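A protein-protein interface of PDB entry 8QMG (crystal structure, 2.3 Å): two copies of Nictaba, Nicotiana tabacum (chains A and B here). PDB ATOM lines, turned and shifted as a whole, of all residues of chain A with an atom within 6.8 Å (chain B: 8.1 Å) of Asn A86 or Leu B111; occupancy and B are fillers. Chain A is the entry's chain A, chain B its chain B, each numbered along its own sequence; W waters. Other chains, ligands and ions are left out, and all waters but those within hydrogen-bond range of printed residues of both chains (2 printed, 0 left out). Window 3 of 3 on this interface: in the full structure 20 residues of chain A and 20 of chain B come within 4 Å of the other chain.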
ATOM      1  N   ARG A  83      12.623 -20.963 -23.790  1.00  0.00           N
ATOM      2  CA  ARG A  83      12.964 -20.162 -22.620  1.00  0.00           C
ATOM      3  C   ARG A  83      11.741 -19.403 -22.126  1.00  0.00           C
ATOM      4  O   ARG A  83      10.790 -19.162 -22.869  1.00  0.00           O
ATOM      5  CB  ARG A  83      14.099 -19.181 -22.937  1.00  0.00           C
ATOM      6  CG  ARG A  83      13.740 -18.166 -23.998  1.00  0.00           C
ATOM      7  CD  ARG A  83      14.958 -17.372 -24.456  1.00  0.00           C
ATOM      8  NE  ARG A  83      14.593 -16.350 -25.430  1.00  0.00           N
ATOM      9  CZ  ARG A  83      15.454 -15.535 -26.019  1.00  0.00           C
ATOM     10  NH1 ARG A  83      16.749 -15.608 -25.767  1.00  0.00           N
ATOM     11  NH2 ARG A  83      15.003 -14.620 -26.880  1.00  0.00           N
ATOM     12  N   PHE A  84      11.775 -19.045 -20.852  1.00  0.00           N
ATOM     13  CA  PHE A  84      10.769 -18.147 -20.303  1.00  0.00           C
ATOM     14  C   PHE A  84      10.994 -16.734 -20.826  1.00  0.00           C
ATOM     15  O   PHE A  84      12.108 -16.209 -20.769  1.00  0.00           O
ATOM     16  CB  PHE A  84      10.822 -18.156 -18.780  1.00  0.00           C
ATOM     17  CG  PHE A  84      10.096 -19.314 -18.156  1.00  0.00           C
ATOM     18  CD1 PHE A  84      10.725 -20.531 -17.974  1.00  0.00           C
ATOM     19  CD2 PHE A  84       8.780 -19.181 -17.752  1.00  0.00           C
ATOM     20  CE1 PHE A  84      10.063 -21.582 -17.404  1.00  0.00           C
ATOM     21  CE2 PHE A  84       8.108 -20.241 -17.186  1.00  0.00           C
ATOM     22  CZ  PHE A  84       8.750 -21.439 -17.009  1.00  0.00           C
ATOM     23  N   VAL A  85       9.927 -16.117 -21.327  1.00  0.00           N
ATOM     24  CA  VAL A  85      10.039 -14.775 -21.890  1.00  0.00           C
ATOM     25  C   VAL A  85      10.611 -13.812 -20.862  1.00  0.00           C
ATOM     26  O   VAL A  85      11.391 -12.919 -21.204  1.00  0.00           O
ATOM     27  CB  VAL A  85       8.666 -14.304 -22.409  1.00  0.00           C
ATOM     28  CG1 VAL A  85       8.708 -12.852 -22.825  1.00  0.00           C
ATOM     29  CG2 VAL A  85       8.222 -15.177 -23.568  1.00  0.00           C
ATOM     30  N   ASN A  86      10.233 -13.972 -19.591  1.00  0.00           N
ATOM     31  CA  ASN A  86      10.648 -13.039 -18.551  1.00  0.00           C
ATOM     32  C   ASN A  86      12.076 -13.270 -18.081  1.00  0.00           C
ATOM     33  O   ASN A  86      12.575 -12.480 -17.270  1.00  0.00           O
ATOM     34  CB  ASN A  86       9.708 -13.122 -17.339  1.00  0.00           C
ATOM     35  CG  ASN A  86       8.287 -12.685 -17.666  1.00  0.00           C
ATOM     36  OD1 ASN A  86       8.041 -12.038 -18.685  1.00  0.00           O
ATOM     37  ND2 ASN A  86       7.351 -13.030 -16.798  1.00  0.00           N
ATOM     38  N   GLU A  87      12.747 -14.315 -18.568  1.00  0.00           N
ATOM     39  CA  GLU A  87      14.121 -14.595 -18.169  1.00  0.00           C
ATOM     40  C   GLU A  87      15.142 -14.186 -19.229  1.00  0.00           C
ATOM     41  O   GLU A  87      16.305 -14.604 -19.159  1.00  0.00           O
ATOM     42  CB  GLU A  87      14.288 -16.077 -17.838  1.00  0.00           C
ATOM     43  CG  GLU A  87      13.559 -16.522 -16.599  1.00  0.00           C
ATOM     44  CD  GLU A  87      13.957 -17.922 -16.155  1.00  0.00           C
ATOM     45  OE1 GLU A  87      14.515 -18.678 -16.976  1.00  0.00           O
ATOM     46  OE2 GLU A  87      13.720 -18.266 -14.976  1.00  0.00           O
ATOM     47  N   VAL A  88      14.738 -13.370 -20.199  1.00  0.00           N
ATOM     48  CA  VAL A  88      15.626 -12.934 -21.274  1.00  0.00           C
ATOM     49  C   VAL A  88      16.283 -11.628 -20.843  1.00  0.00           C
ATOM     50  O   VAL A  88      15.615 -10.598 -20.693  1.00  0.00           O
ATOM     51  CB  VAL A  88      14.870 -12.766 -22.598  1.00  0.00           C
ATOM     52  CG1 VAL A  88      15.801 -12.266 -23.686  1.00  0.00           C
ATOM     53  CG2 VAL A  88      14.205 -14.072 -23.004  1.00  0.00           C
ATOM     54  N   ALA A  89      17.598 -11.668 -20.643  1.00  0.00           N
ATOM     55  CA  ALA A  89      18.327 -10.476 -20.240  1.00  0.00           C
ATOM     56  C   ALA A  89      18.338  -9.452 -21.368  1.00  0.00           C
ATOM     57  O   ALA A  89      18.449  -9.799 -22.548  1.00  0.00           O
ATOM     58  CB  ALA A  89      19.761 -10.827 -19.848  1.00  0.00           C
ATOM     59  N   GLU A  90      18.224  -8.181 -20.993  1.00  0.00           N
ATOM     60  CA  GLU A  90      18.248  -7.107 -21.974  1.00  0.00           C
ATOM     61  C   GLU A  90      19.471  -7.224 -22.876  1.00  0.00           C
ATOM     62  O   GLU A  90      20.609  -7.304 -22.398  1.00  0.00           O
ATOM     63  CB  GLU A  90      18.256  -5.759 -21.262  1.00  0.00           C
ATOM     64  CG  GLU A  90      18.365  -4.566 -22.198  1.00  0.00           C
ATOM     65  CD  GLU A  90      18.045  -3.256 -21.510  1.00  0.00           C
ATOM     66  OE1 GLU A  90      18.865  -2.781 -20.698  1.00  0.00           O
ATOM     67  OE2 GLU A  90      16.953  -2.717 -21.772  1.00  0.00           O
ATOM     68  N   GLU A 136       2.650 -18.814 -12.730  1.00  0.00           N
ATOM     69  CA  GLU A 136       2.819 -17.382 -12.530  1.00  0.00           C
ATOM     70  C   GLU A 136       4.139 -16.845 -13.073  1.00  0.00           C
ATOM     71  O   GLU A 136       4.428 -15.653 -12.906  1.00  0.00           O
ATOM     72  CB  GLU A 136       2.713 -17.047 -11.037  1.00  0.00           C
ATOM     73  CG  GLU A 136       1.384 -17.420 -10.397  1.00  0.00           C
ATOM     74  CD  GLU A 136       1.368 -17.144  -8.893  1.00  0.00           C
ATOM     75  OE1 GLU A 136       2.421 -16.728  -8.348  1.00  0.00           O
ATOM     76  OE2 GLU A 136       0.304 -17.338  -8.258  1.00  0.00           O
ATOM     77  N   ASP A 137       4.954 -17.687 -13.699  1.00  0.00           N
ATOM     78  CA  ASP A 137       6.234 -17.259 -14.249  1.00  0.00           C
ATOM     79  C   ASP A 137       6.105 -16.713 -15.668  1.00  0.00           C
ATOM     80  O   ASP A 137       7.123 -16.398 -16.298  1.00  0.00           O
ATOM     81  CB  ASP A 137       7.234 -18.422 -14.212  1.00  0.00           C
ATOM     82  CG  ASP A 137       7.637 -18.802 -12.789  1.00  0.00           C
ATOM     83  OD1 ASP A 137       7.976 -17.889 -12.001  1.00  0.00           O
ATOM     84  OD2 ASP A 137       7.581 -20.004 -12.451  1.00  0.00           O
ATOM     85  N   GLY A 138       4.885 -16.602 -16.190  1.00  0.00           N
ATOM     86  CA  GLY A 138       4.687 -15.982 -17.483  1.00  0.00           C
ATOM     87  C   GLY A 138       4.674 -16.945 -18.647  1.00  0.00           C
ATOM     88  O   GLY A 138       4.325 -18.116 -18.492  1.00  0.00           O
ATOM     89  N   GLU A 139       5.058 -16.455 -19.821  1.00  0.00           N
ATOM     90  CA  GLU A 139       4.996 -17.249 -21.036  1.00  0.00           C
ATOM     91  C   GLU A 139       6.319 -17.965 -21.310  1.00  0.00           C
ATOM     92  O   GLU A 139       7.376 -17.606 -20.787  1.00  0.00           O
ATOM     93  CB  GLU A 139       4.627 -16.366 -22.232  1.00  0.00           C
ATOM     94  CG  GLU A 139       3.661 -15.261 -21.895  1.00  0.00           C
ATOM     95  CD  GLU A 139       3.004 -14.641 -23.126  1.00  0.00           C
ATOM     96  OE1 GLU A 139       3.636 -13.828 -23.832  1.00  0.00           O
ATOM     97  OE2 GLU A 139       1.847 -14.993 -23.376  1.00  0.00           O
ATOM     98  N   ARG B  77      27.021  -9.498 -15.454  1.00  0.00           N
ATOM     99  CA  ARG B  77      26.451 -10.573 -16.248  1.00  0.00           C
ATOM    100  C   ARG B  77      27.465 -11.698 -16.398  1.00  0.00           C
ATOM    101  O   ARG B  77      28.673 -11.506 -16.237  1.00  0.00           O
ATOM    102  CB  ARG B  77      26.032 -10.096 -17.643  1.00  0.00           C
ATOM    103  CG  ARG B  77      25.036  -8.961 -17.647  1.00  0.00           C
ATOM    104  CD  ARG B  77      24.708  -8.554 -19.068  1.00  0.00           C
ATOM    105  NE  ARG B  77      23.543  -7.682 -19.125  1.00  0.00           N
ATOM    106  CZ  ARG B  77      22.726  -7.602 -20.164  1.00  0.00           C
ATOM    107  NH1 ARG B  77      22.911  -8.350 -21.243  1.00  0.00           N
ATOM    108  NH2 ARG B  77      21.692  -6.765 -20.114  1.00  0.00           N
ATOM    109  N   THR B  98      22.538 -15.910 -20.935  1.00  0.00           N
ATOM    110  CA  THR B  98      22.989 -14.794 -20.123  1.00  0.00           C
ATOM    111  C   THR B  98      22.167 -14.708 -18.839  1.00  0.00           C
ATOM    112  O   THR B  98      20.931 -14.706 -18.878  1.00  0.00           O
ATOM    113  CB  THR B  98      22.868 -13.485 -20.903  1.00  0.00           C
ATOM    114  OG1 THR B  98      23.620 -13.552 -22.122  1.00  0.00           O
ATOM    115  CG2 THR B  98      23.389 -12.325 -20.062  1.00  0.00           C
ATOM    116  N   PHE B 100      22.286 -12.758 -14.676  1.00  0.00           N
ATOM    117  CA  PHE B 100      22.841 -11.706 -13.840  1.00  0.00           C
ATOM    118  C   PHE B 100      23.439 -12.317 -12.577  1.00  0.00           C
ATOM    119  O   PHE B 100      22.925 -13.302 -12.040  1.00  0.00           O
ATOM    120  CB  PHE B 100      21.771 -10.668 -13.493  1.00  0.00           C
ATOM    121  CG  PHE B 100      21.258  -9.908 -14.686  1.00  0.00           C
ATOM    122  CD1 PHE B 100      22.087  -9.046 -15.382  1.00  0.00           C
ATOM    123  CD2 PHE B 100      19.952 -10.054 -15.107  1.00  0.00           C
ATOM    124  CE1 PHE B 100      21.627  -8.352 -16.476  1.00  0.00           C
ATOM    125  CE2 PHE B 100      19.482  -9.362 -16.195  1.00  0.00           C
ATOM    126  CZ  PHE B 100      20.314  -8.509 -16.885  1.00  0.00           C
ATOM    127  N   LYS B 103      24.688  -7.809 -10.582  1.00  0.00           N
ATOM    128  CA  LYS B 103      23.670  -6.794 -10.819  1.00  0.00           C
ATOM    129  C   LYS B 103      22.444  -7.051  -9.948  1.00  0.00           C
ATOM    130  O   LYS B 103      22.006  -8.192  -9.780  1.00  0.00           O
ATOM    131  CB  LYS B 103      23.271  -6.781 -12.292  1.00  0.00           C
ATOM    132  CG  LYS B 103      22.522  -5.529 -12.721  1.00  0.00           C
ATOM    133  CD  LYS B 103      21.959  -5.692 -14.132  1.00  0.00           C
ATOM    134  CE  LYS B 103      21.145  -4.485 -14.544  1.00  0.00           C
ATOM    135  NZ  LYS B 103      19.984  -4.265 -13.640  1.00  0.00           N
ATOM    136  N   LYS B 105      18.423  -6.532  -9.175  1.00  0.00           N
ATOM    137  CA  LYS B 105      17.149  -6.326  -9.864  1.00  0.00           C
ATOM    138  C   LYS B 105      16.485  -5.093  -9.260  1.00  0.00           C
ATOM    139  O   LYS B 105      15.798  -5.164  -8.238  1.00  0.00           O
ATOM    140  CB  LYS B 105      16.280  -7.565  -9.720  1.00  0.00           C
ATOM    141  CG  LYS B 105      14.974  -7.513 -10.497  1.00  0.00           C
ATOM    142  CD  LYS B 105      14.251  -8.861 -10.410  1.00  0.00           C
ATOM    143  CE  LYS B 105      12.925  -8.847 -11.162  1.00  0.00           C
ATOM    144  NZ  LYS B 105      11.910  -7.990 -10.500  1.00  0.00           N
ATOM    145  N   LEU B 107      14.228  -2.993 -10.887  1.00  0.00           N
ATOM    146  CA  LEU B 107      12.869  -2.783 -11.348  1.00  0.00           C
ATOM    147  C   LEU B 107      12.054  -4.060 -11.180  1.00  0.00           C
ATOM    148  O   LEU B 107      12.541  -5.147 -11.512  1.00  0.00           O
ATOM    149  CB  LEU B 107      12.854  -2.371 -12.825  1.00  0.00           C
ATOM    150  CG  LEU B 107      13.544  -1.104 -13.323  1.00  0.00           C
ATOM    151  CD1 LEU B 107      12.708   0.125 -12.986  1.00  0.00           C
ATOM    152  CD2 LEU B 107      14.947  -0.960 -12.768  1.00  0.00           C
ATOM    153  N   PRO B 108      10.811  -3.973 -10.696  1.00  0.00           N
ATOM    154  CA  PRO B 108       9.981  -5.192 -10.612  1.00  0.00           C
ATOM    155  C   PRO B 108       9.690  -5.819 -11.964  1.00  0.00           C
ATOM    156  O   PRO B 108       9.432  -7.027 -12.023  1.00  0.00           O
ATOM    157  CB  PRO B 108       8.694  -4.710  -9.923  1.00  0.00           C
ATOM    158  CG  PRO B 108       8.660  -3.220 -10.166  1.00  0.00           C
ATOM    159  CD  PRO B 108      10.108  -2.779 -10.184  1.00  0.00           C
ATOM    160  N   GLY B 109       9.724  -5.042 -13.046  1.00  0.00           N
ATOM    161  CA  GLY B 109       9.458  -5.571 -14.368  1.00  0.00           C
ATOM    162  C   GLY B 109      10.707  -5.840 -15.186  1.00  0.00           C
ATOM    163  O   GLY B 109      10.634  -6.022 -16.405  1.00  0.00           O
ATOM    164  N   GLU B 110      11.862  -5.870 -14.530  1.00  0.00           N
ATOM    165  CA  GLU B 110      13.111  -6.126 -15.235  1.00  0.00           C
ATOM    166  C   GLU B 110      13.198  -7.600 -15.606  1.00  0.00           C
ATOM    167  O   GLU B 110      12.922  -8.474 -14.780  1.00  0.00           O
ATOM    168  CB  GLU B 110      14.301  -5.714 -14.375  1.00  0.00           C
ATOM    169  CG  GLU B 110      15.590  -5.550 -15.170  1.00  0.00           C
ATOM    170  CD  GLU B 110      16.735  -5.023 -14.319  1.00  0.00           C
ATOM    171  OE1 GLU B 110      16.474  -4.550 -13.189  1.00  0.00           O
ATOM    172  OE2 GLU B 110      17.895  -5.090 -14.781  1.00  0.00           O
ATOM    173  N   LEU B 111      13.589  -7.875 -16.843  1.00  0.00           N
ATOM    174  CA  LEU B 111      13.648  -9.237 -17.343  1.00  0.00           C
ATOM    175  C   LEU B 111      15.029  -9.840 -17.112  1.00  0.00           C
ATOM    176  O   LEU B 111      16.045  -9.135 -17.060  1.00  0.00           O
ATOM    177  CB  LEU B 111      13.302  -9.267 -18.831  1.00  0.00           C
ATOM    178  CG  LEU B 111      11.964  -8.645 -19.226  1.00  0.00           C
ATOM    179  CD1 LEU B 111      11.583  -9.073 -20.627  1.00  0.00           C
ATOM    180  CD2 LEU B 111      10.881  -9.020 -18.244  1.00  0.00           C
ATOM    181  N   GLY B 112      15.053 -11.161 -16.969  1.00  0.00           N
ATOM    182  CA  GLY B 112      16.289 -11.885 -16.767  1.00  0.00           C
ATOM    183  C   GLY B 112      16.268 -12.741 -15.521  1.00  0.00           C
ATOM    184  O   GLY B 112      15.436 -12.528 -14.635  1.00  0.00           O
ATOM    185  N   ARG B 113      17.176 -13.714 -15.442  1.00  0.00           N
ATOM    186  CA  ARG B 113      17.360 -14.518 -14.241  1.00  0.00           C
ATOM    187  C   ARG B 113      18.341 -13.802 -13.313  1.00  0.00           C
ATOM    188  O   ARG B 113      19.503 -13.588 -13.673  1.00  0.00           O
ATOM    189  CB  ARG B 113      17.873 -15.919 -14.580  1.00  0.00           C
ATOM    190  CG  ARG B 113      16.828 -16.830 -15.168  1.00  0.00           C
ATOM    191  CD  ARG B 113      16.992 -18.263 -14.665  1.00  0.00           C
ATOM    192  NE  ARG B 113      18.178 -18.921 -15.194  1.00  0.00           N
ATOM    193  CZ  ARG B 113      18.195 -19.644 -16.305  1.00  0.00           C
ATOM    194  NH1 ARG B 113      17.100 -19.828 -17.025  1.00  0.00           N
ATOM    195  NH2 ARG B 113      19.339 -20.193 -16.706  1.00  0.00           N
ATOM    196  N   PHE B 114      17.880 -13.450 -12.124  1.00  0.00           N
ATOM    197  CA  PHE B 114      18.711 -12.839 -11.093  1.00  0.00           C
ATOM    198  C   PHE B 114      18.965 -13.827  -9.961  1.00  0.00           C
ATOM    199  O   PHE B 114      18.249 -14.824  -9.818  1.00  0.00           O
ATOM    200  CB  PHE B 114      18.047 -11.577 -10.518  1.00  0.00           C
ATOM    201  CG  PHE B 114      18.000 -10.421 -11.479  1.00  0.00           C
ATOM    202  CD1 PHE B 114      17.018 -10.348 -12.457  1.00  0.00           C
ATOM    203  CD2 PHE B 114      18.934  -9.404 -11.398  1.00  0.00           C
ATOM    204  CE1 PHE B 114      16.975  -9.281 -13.342  1.00  0.00           C
ATOM    205  CE2 PHE B 114      18.894  -8.339 -12.273  1.00  0.00           C
ATOM    206  CZ  PHE B 114      17.910  -8.277 -13.249  1.00  0.00           C
HETATM  207  O   HOH W   1      19.370 -14.310 -21.158  1.00  0.00           O
HETATM  208  O   HOH W   2      18.754 -14.342 -17.756  1.00  0.00           O
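O of Asn A86 sits at hydrogen-bond distance from N of Gly B112, 2.8 Å away.
The guanidinium group of Arg B113 is in salt-bridge range of the side-chain carboxylate of Glu A87 (2.8 Å).
The backbone carbonyl oxygen (O) of Glu A90 lies within hydrogen-bond range of the guanidinium group (NH2) of Arg B77 (2.6 Å).
The backbone NH (N) of Val A85 sits at hydrogen-bond distance from the backbone carbonyl oxygen (O) of Glu A139, 3.0 Å away.
The side-chain amide nitrogen of Asn A86 sits at hydrogen-bond distance from the backbone carbonyl oxygen of Asp A137, 3.4 Å away.
N of Phe B100 is in hydrogen-bond range of O of Arg B113.
Val A85 touches Leu B111.
Leu B111 touches Asn A86.
Gly B112 touches Glu A87.
Val A88 touches Leu B111 (O to CB, 3.3 Å).
O of Val A88 touches N of Gly B112, 3.8 Å away.
Ala A89 touches Thr B98 (CB to CG2, 3.9 Å).
Ala A89 touches Phe B100 (CB to CZ, 3.8 Å).
Asn A86 touches just these residues of chain B: Leu B111 and Gly B112.
Glu A139 touches none of the printed residues of chain B.
Of the printed residues of chain A, Phe B100 touches Ala A89.
Lys B103 touches none of the printed residues of chain A.
Printed residues of chain A within 4 Å of Leu B111: Val A85 (3.9 Å), Asn A86 (3.4 Å) and Val A88 (3.3 Å).
Printed residues of chain A within 4 Å of Arg B113: Glu A87 (2.8 Å).
The nearest residue of chain B that does not touch Asn A86 is Glu B110 (4.7 Å).
The nearest residue of chain A that does not touch Leu B111 is Ala A89 (4.1 Å).
The nearest printed residue of chain A that does not touch Arg B113 is Asn A86 (5.1 Å).
Of the 12 printed residues of chain A, 6 touch a printed residue of chain B.
Hydrophobic or aromatic side chains of chain A that line the printed part of chain B: Ala A89.
Hydrophobic or aromatic side chains of chain B that line the printed part of chain A: Phe B100 and Leu B111.
Among the printed residues, 10 pairs touch across the chains.
Among the printed residues, Asp or Glu carboxylates within 4 Å of a Lys or Arg side-chain nitrogen of the other chain: Glu A87 with Arg B113 (2.8 Å).
No position is printed for both chains.
Of the 10 pairs that touch across the chains among the printed residues, none has its exchanged pair printed and touching as well.
Water W2 lies within hydrogen-bond range of the backbone carbonyl oxygen (O) of Thr B98 (2.5 Å), the backbone carbonyl oxygen (O) of Glu A87 (2.8 Å) and the backbone NH (N) of Arg B113 (2.9 Å).
Water W1 bridges the backbone carbonyl oxygen (O) of Thr B98 (2.8 Å) and the backbone NH (N) of Ala A89 (3.2 Å).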
